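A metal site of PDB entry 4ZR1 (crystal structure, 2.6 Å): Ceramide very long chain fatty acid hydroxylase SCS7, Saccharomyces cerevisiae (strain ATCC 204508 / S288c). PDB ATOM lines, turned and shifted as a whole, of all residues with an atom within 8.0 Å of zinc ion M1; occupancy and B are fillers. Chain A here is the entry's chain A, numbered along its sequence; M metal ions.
Of the 18 residues printed, 5 come within 4 Å of zinc ion M1.
Zinc ion M1 is bound by a ring nitrogen (NE2) of His 255 (2.0 Å), a ring nitrogen (NE2) of His 236 (2.1 Å), a ring nitrogen (NE2) of His 251 (2.2 Å), a ring nitrogen (NE2) of His 177 (2.3 Å) and a ring nitrogen (NE2) of His 232 (2.3 Å). Zinc ion M1 has five donor atoms within binding distance.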
ATOM      1  N   HIS A 150      -3.750 -26.993  16.758  1.00  0.00           N
ATOM      2  CA  HIS A 150      -5.016 -26.937  16.046  1.00  0.00           C
ATOM      3  C   HIS A 150      -5.380 -28.277  15.434  1.00  0.00           C
ATOM      4  O   HIS A 150      -6.504 -28.754  15.597  1.00  0.00           O
ATOM      5  CB  HIS A 150      -4.979 -25.876  14.972  1.00  0.00           C
ATOM      6  CG  HIS A 150      -6.318 -25.577  14.385  1.00  0.00           C
ATOM      7  ND1 HIS A 150      -6.502 -24.745  13.298  1.00  0.00           N
ATOM      8  CD2 HIS A 150      -7.554 -26.010  14.745  1.00  0.00           C
ATOM      9  CE1 HIS A 150      -7.791 -24.685  13.006  1.00  0.00           C
ATOM     10  NE2 HIS A 150      -8.452 -25.437  13.866  1.00  0.00           N
ATOM     11  N   HIS A 174     -11.753 -26.060  21.895  1.00  0.00           N
ATOM     12  CA  HIS A 174     -11.971 -25.695  20.503  1.00  0.00           C
ATOM     13  C   HIS A 174     -13.375 -26.039  19.974  1.00  0.00           C
ATOM     14  O   HIS A 174     -13.901 -25.356  19.101  1.00  0.00           O
ATOM     15  CB  HIS A 174     -10.922 -26.351  19.631  1.00  0.00           C
ATOM     16  CG  HIS A 174     -10.795 -25.740  18.275  1.00  0.00           C
ATOM     17  ND1 HIS A 174     -10.445 -24.421  18.081  1.00  0.00           N
ATOM     18  CD2 HIS A 174     -10.988 -26.260  17.039  1.00  0.00           C
ATOM     19  CE1 HIS A 174     -10.419 -24.156  16.791  1.00  0.00           C
ATOM     20  NE2 HIS A 174     -10.743 -25.260  16.133  1.00  0.00           N
ATOM     21  N   HIS A 177     -15.978 -23.312  19.892  1.00  0.00           N
ATOM     22  CA  HIS A 177     -15.743 -22.304  18.883  1.00  0.00           C
ATOM     23  C   HIS A 177     -16.315 -22.764  17.523  1.00  0.00           C
ATOM     24  O   HIS A 177     -16.857 -21.956  16.760  1.00  0.00           O
ATOM     25  CB  HIS A 177     -14.252 -21.986  18.790  1.00  0.00           C
ATOM     26  CG  HIS A 177     -13.920 -21.046  17.680  1.00  0.00           C
ATOM     27  ND1 HIS A 177     -14.464 -19.780  17.595  1.00  0.00           N
ATOM     28  CD2 HIS A 177     -13.148 -21.197  16.586  1.00  0.00           C
ATOM     29  CE1 HIS A 177     -14.013 -19.190  16.498  1.00  0.00           C
ATOM     30  NE2 HIS A 177     -13.219 -20.025  15.873  1.00  0.00           N
ATOM     31  N   HIS A 178     -16.210 -24.054  17.236  1.00  0.00           N
ATOM     32  CA  HIS A 178     -16.820 -24.601  16.028  1.00  0.00           C
ATOM     33  C   HIS A 178     -18.331 -24.673  16.174  1.00  0.00           C
ATOM     34  O   HIS A 178     -19.072 -24.464  15.209  1.00  0.00           O
ATOM     35  CB  HIS A 178     -16.262 -25.991  15.723  1.00  0.00           C
ATOM     36  CG  HIS A 178     -15.033 -25.969  14.863  1.00  0.00           C
ATOM     37  ND1 HIS A 178     -15.049 -26.301  13.535  1.00  0.00           N
ATOM     38  CD2 HIS A 178     -13.755 -25.636  15.156  1.00  0.00           C
ATOM     39  CE1 HIS A 178     -13.825 -26.182  13.033  1.00  0.00           C
ATOM     40  NE2 HIS A 178     -13.029 -25.778  14.001  1.00  0.00           N
ATOM     41  N   PRO A 181     -19.136 -20.209  16.157  1.00  0.00           N
ATOM     42  CA  PRO A 181     -18.125 -19.415  15.441  1.00  0.00           C
ATOM     43  C   PRO A 181     -18.239 -17.899  15.674  1.00  0.00           C
ATOM     44  O   PRO A 181     -17.229 -17.219  15.871  1.00  0.00           O
ATOM     45  CB  PRO A 181     -18.409 -19.731  13.979  1.00  0.00           C
ATOM     46  CG  PRO A 181     -19.151 -21.006  13.978  1.00  0.00           C
ATOM     47  CD  PRO A 181     -19.959 -21.006  15.220  1.00  0.00           C
ATOM     48  N   MET A 182     -19.462 -17.383  15.662  1.00  0.00           N
ATOM     49  CA  MET A 182     -19.693 -15.951  15.795  1.00  0.00           C
ATOM     50  C   MET A 182     -19.991 -15.489  17.211  1.00  0.00           C
ATOM     51  O   MET A 182     -20.487 -14.382  17.408  1.00  0.00           O
ATOM     52  CB  MET A 182     -20.829 -15.511  14.883  1.00  0.00           C
ATOM     53  CG  MET A 182     -20.431 -15.505  13.432  1.00  0.00           C
ATOM     54  SD  MET A 182     -18.986 -14.448  13.191  1.00  0.00           S
ATOM     55  CE  MET A 182     -18.028 -15.509  12.107  1.00  0.00           C
ATOM     56  N   LEU A 187     -14.083 -16.855  21.381  1.00  0.00           N
ATOM     57  CA  LEU A 187     -13.164 -17.124  20.293  1.00  0.00           C
ATOM     58  C   LEU A 187     -11.735 -17.169  20.824  1.00  0.00           C
ATOM     59  O   LEU A 187     -11.084 -18.217  20.773  1.00  0.00           O
ATOM     60  CB  LEU A 187     -13.325 -16.084  19.188  1.00  0.00           C
ATOM     61  CG  LEU A 187     -12.609 -16.286  17.859  1.00  0.00           C
ATOM     62  CD1 LEU A 187     -13.253 -15.480  16.740  1.00  0.00           C
ATOM     63  CD2 LEU A 187     -11.145 -15.895  17.978  1.00  0.00           C
ATOM     64  N   TYR A 228      -1.604 -14.571  16.522  1.00  0.00           N
ATOM     65  CA  TYR A 228      -2.542 -15.625  16.122  1.00  0.00           C
ATOM     66  C   TYR A 228      -3.996 -15.391  16.576  1.00  0.00           C
ATOM     67  O   TYR A 228      -4.924 -15.432  15.763  1.00  0.00           O
ATOM     68  CB  TYR A 228      -2.067 -16.982  16.658  1.00  0.00           C
ATOM     69  CG  TYR A 228      -3.199 -17.972  16.855  1.00  0.00           C
ATOM     70  CD1 TYR A 228      -3.725 -18.683  15.782  1.00  0.00           C
ATOM     71  CD2 TYR A 228      -3.743 -18.211  18.115  1.00  0.00           C
ATOM     72  CE1 TYR A 228      -4.763 -19.590  15.951  1.00  0.00           C
ATOM     73  CE2 TYR A 228      -4.759 -19.110  18.304  1.00  0.00           C
ATOM     74  CZ  TYR A 228      -5.277 -19.793  17.207  1.00  0.00           C
ATOM     75  OH  TYR A 228      -6.306 -20.695  17.393  1.00  0.00           O
ATOM     76  N   HIS A 232      -6.989 -14.533  14.470  1.00  0.00           N
ATOM     77  CA  HIS A 232      -8.111 -15.459  14.524  1.00  0.00           C
ATOM     78  C   HIS A 232      -9.430 -14.735  14.778  1.00  0.00           C
ATOM     79  O   HIS A 232     -10.406 -14.967  14.085  1.00  0.00           O
ATOM     80  CB  HIS A 232      -7.900 -16.508  15.594  1.00  0.00           C
ATOM     81  CG  HIS A 232      -8.947 -17.566  15.603  1.00  0.00           C
ATOM     82  ND1 HIS A 232      -9.154 -18.397  16.683  1.00  0.00           N
ATOM     83  CD2 HIS A 232      -9.844 -17.930  14.664  1.00  0.00           C
ATOM     84  CE1 HIS A 232     -10.148 -19.228  16.396  1.00  0.00           C
ATOM     85  NE2 HIS A 232     -10.592 -18.957  15.186  1.00  0.00           N
ATOM     86  N   PHE A 233      -9.436 -13.846  15.770  1.00  0.00           N
ATOM     87  CA  PHE A 233     -10.622 -13.042  16.047  1.00  0.00           C
ATOM     88  C   PHE A 233     -11.094 -12.260  14.822  1.00  0.00           C
ATOM     89  O   PHE A 233     -12.262 -12.353  14.444  1.00  0.00           O
ATOM     90  CB  PHE A 233     -10.365 -12.061  17.200  1.00  0.00           C
ATOM     91  CG  PHE A 233     -11.602 -11.360  17.664  1.00  0.00           C
ATOM     92  CD1 PHE A 233     -12.452 -11.975  18.592  1.00  0.00           C
ATOM     93  CD2 PHE A 233     -11.949 -10.107  17.165  1.00  0.00           C
ATOM     94  CE1 PHE A 233     -13.616 -11.343  19.016  1.00  0.00           C
ATOM     95  CE2 PHE A 233     -13.124  -9.466  17.592  1.00  0.00           C
ATOM     96  CZ  PHE A 233     -13.947 -10.079  18.505  1.00  0.00           C
ATOM     97  N   LEU A 235     -10.509 -12.472  11.738  1.00  0.00           N
ATOM     98  CA  LEU A 235     -10.937 -13.288  10.624  1.00  0.00           C
ATOM     99  C   LEU A 235     -12.447 -13.559  10.666  1.00  0.00           C
ATOM    100  O   LEU A 235     -13.101 -13.638   9.640  1.00  0.00           O
ATOM    101  CB  LEU A 235     -10.175 -14.611  10.600  1.00  0.00           C
ATOM    102  CG  LEU A 235      -8.711 -14.595  10.193  1.00  0.00           C
ATOM    103  CD1 LEU A 235      -8.231 -16.028  10.035  1.00  0.00           C
ATOM    104  CD2 LEU A 235      -8.514 -13.812   8.899  1.00  0.00           C
ATOM    105  N   HIS A 236     -12.993 -13.696  11.872  1.00  0.00           N
ATOM    106  CA  HIS A 236     -14.426 -13.958  12.035  1.00  0.00           C
ATOM    107  C   HIS A 236     -15.252 -12.682  12.083  1.00  0.00           C
ATOM    108  O   HIS A 236     -16.339 -12.609  11.494  1.00  0.00           O
ATOM    109  CB  HIS A 236     -14.697 -14.757  13.315  1.00  0.00           C
ATOM    110  CG  HIS A 236     -14.336 -16.200  13.211  1.00  0.00           C
ATOM    111  ND1 HIS A 236     -15.171 -17.128  12.637  1.00  0.00           N
ATOM    112  CD2 HIS A 236     -13.231 -16.881  13.617  1.00  0.00           C
ATOM    113  CE1 HIS A 236     -14.595 -18.324  12.683  1.00  0.00           C
ATOM    114  NE2 HIS A 236     -13.420 -18.195  13.269  1.00  0.00           N
ATOM    115  N   HIS A 251      -9.826 -19.549   6.274  1.00  0.00           N
ATOM    116  CA  HIS A 251     -10.143 -20.011   7.613  1.00  0.00           C
ATOM    117  C   HIS A 251     -11.623 -20.288   7.794  1.00  0.00           C
ATOM    118  O   HIS A 251     -12.011 -21.266   8.440  1.00  0.00           O
ATOM    119  CB  HIS A 251      -9.689 -18.989   8.650  1.00  0.00           C
ATOM    120  CG  HIS A 251     -10.089 -19.351  10.037  1.00  0.00           C
ATOM    121  ND1 HIS A 251      -9.562 -20.443  10.697  1.00  0.00           N
ATOM    122  CD2 HIS A 251     -11.001 -18.813  10.873  1.00  0.00           C
ATOM    123  CE1 HIS A 251     -10.119 -20.545  11.886  1.00  0.00           C
ATOM    124  NE2 HIS A 251     -10.991 -19.568  12.027  1.00  0.00           N
ATOM    125  N   LEU A 252     -12.463 -19.440   7.221  1.00  0.00           N
ATOM    126  CA  LEU A 252     -13.901 -19.617   7.302  1.00  0.00           C
ATOM    127  C   LEU A 252     -14.328 -20.917   6.641  1.00  0.00           C
ATOM    128  O   LEU A 252     -15.324 -21.526   7.047  1.00  0.00           O
ATOM    129  CB  LEU A 252     -14.629 -18.432   6.660  1.00  0.00           C
ATOM    130  CG  LEU A 252     -15.245 -17.411   7.613  1.00  0.00           C
ATOM    131  CD1 LEU A 252     -14.355 -17.129   8.804  1.00  0.00           C
ATOM    132  CD2 LEU A 252     -15.517 -16.123   6.876  1.00  0.00           C
ATOM    133  N   HIS A 254     -12.579 -23.573   6.797  1.00  0.00           N
ATOM    134  CA  HIS A 254     -12.258 -24.565   7.803  1.00  0.00           C
ATOM    135  C   HIS A 254     -13.466 -24.778   8.723  1.00  0.00           C
ATOM    136  O   HIS A 254     -13.686 -25.862   9.268  1.00  0.00           O
ATOM    137  CB  HIS A 254     -11.045 -24.140   8.617  1.00  0.00           C
ATOM    138  CG  HIS A 254     -10.853 -24.925   9.872  1.00  0.00           C
ATOM    139  ND1 HIS A 254     -10.184 -26.139   9.898  1.00  0.00           N
ATOM    140  CD2 HIS A 254     -11.262 -24.702  11.140  1.00  0.00           C
ATOM    141  CE1 HIS A 254     -10.195 -26.612  11.128  1.00  0.00           C
ATOM    142  NE2 HIS A 254     -10.841 -25.759  11.903  1.00  0.00           N
ATOM    143  N   HIS A 255     -14.249 -23.729   8.889  1.00  0.00           N
ATOM    144  CA  HIS A 255     -15.448 -23.756   9.700  1.00  0.00           C
ATOM    145  C   HIS A 255     -16.663 -24.285   8.931  1.00  0.00           C
ATOM    146  O   HIS A 255     -17.341 -25.211   9.385  1.00  0.00           O
ATOM    147  CB  HIS A 255     -15.740 -22.345  10.222  1.00  0.00           C
ATOM    148  CG  HIS A 255     -14.897 -21.949  11.402  1.00  0.00           C
ATOM    149  ND1 HIS A 255     -15.128 -22.432  12.668  1.00  0.00           N
ATOM    150  CD2 HIS A 255     -13.840 -21.117  11.493  1.00  0.00           C
ATOM    151  CE1 HIS A 255     -14.228 -21.924  13.503  1.00  0.00           C
ATOM    152  NE2 HIS A 255     -13.442 -21.112  12.816  1.00  0.00           N
ATOM    153  N   TYR A 256     -16.943 -23.715   7.765  1.00  0.00           N
ATOM    154  CA  TYR A 256     -18.199 -23.985   7.078  1.00  0.00           C
ATOM    155  C   TYR A 256     -18.083 -24.859   5.826  1.00  0.00           C
ATOM    156  O   TYR A 256     -18.973 -24.837   4.985  1.00  0.00           O
ATOM    157  CB  TYR A 256     -18.857 -22.661   6.684  1.00  0.00           C
ATOM    158  CG  TYR A 256     -18.995 -21.681   7.821  1.00  0.00           C
ATOM    159  CD1 TYR A 256     -20.093 -21.729   8.691  1.00  0.00           C
ATOM    160  CD2 TYR A 256     -18.046 -20.688   8.024  1.00  0.00           C
ATOM    161  CE1 TYR A 256     -20.223 -20.821   9.730  1.00  0.00           C
ATOM    162  CE2 TYR A 256     -18.171 -19.792   9.051  1.00  0.00           C
ATOM    163  CZ  TYR A 256     -19.253 -19.851   9.905  1.00  0.00           C
ATOM    164  OH  TYR A 256     -19.353 -18.944  10.916  1.00  0.00           O
ATOM    165  N   VAL A 265      -3.964 -20.697  10.575  1.00  0.00           N
ATOM    166  CA  VAL A 265      -4.889 -19.570  10.592  1.00  0.00           C
ATOM    167  C   VAL A 265      -4.141 -18.241  10.502  1.00  0.00           C
ATOM    168  O   VAL A 265      -4.712 -17.237  10.045  1.00  0.00           O
ATOM    169  CB  VAL A 265      -5.861 -19.613  11.862  1.00  0.00           C
ATOM    170  CG1 VAL A 265      -5.771 -20.945  12.592  1.00  0.00           C
ATOM    171  CG2 VAL A 265      -5.630 -18.472  12.816  1.00  0.00           C
HETATM  172 ZN    ZN M   1     -12.248 -19.825  13.840  1.00  0.00          ZN
HETATM  173 ZN    ZN M   2     -10.720 -25.832  14.051  1.00  0.00          ZN
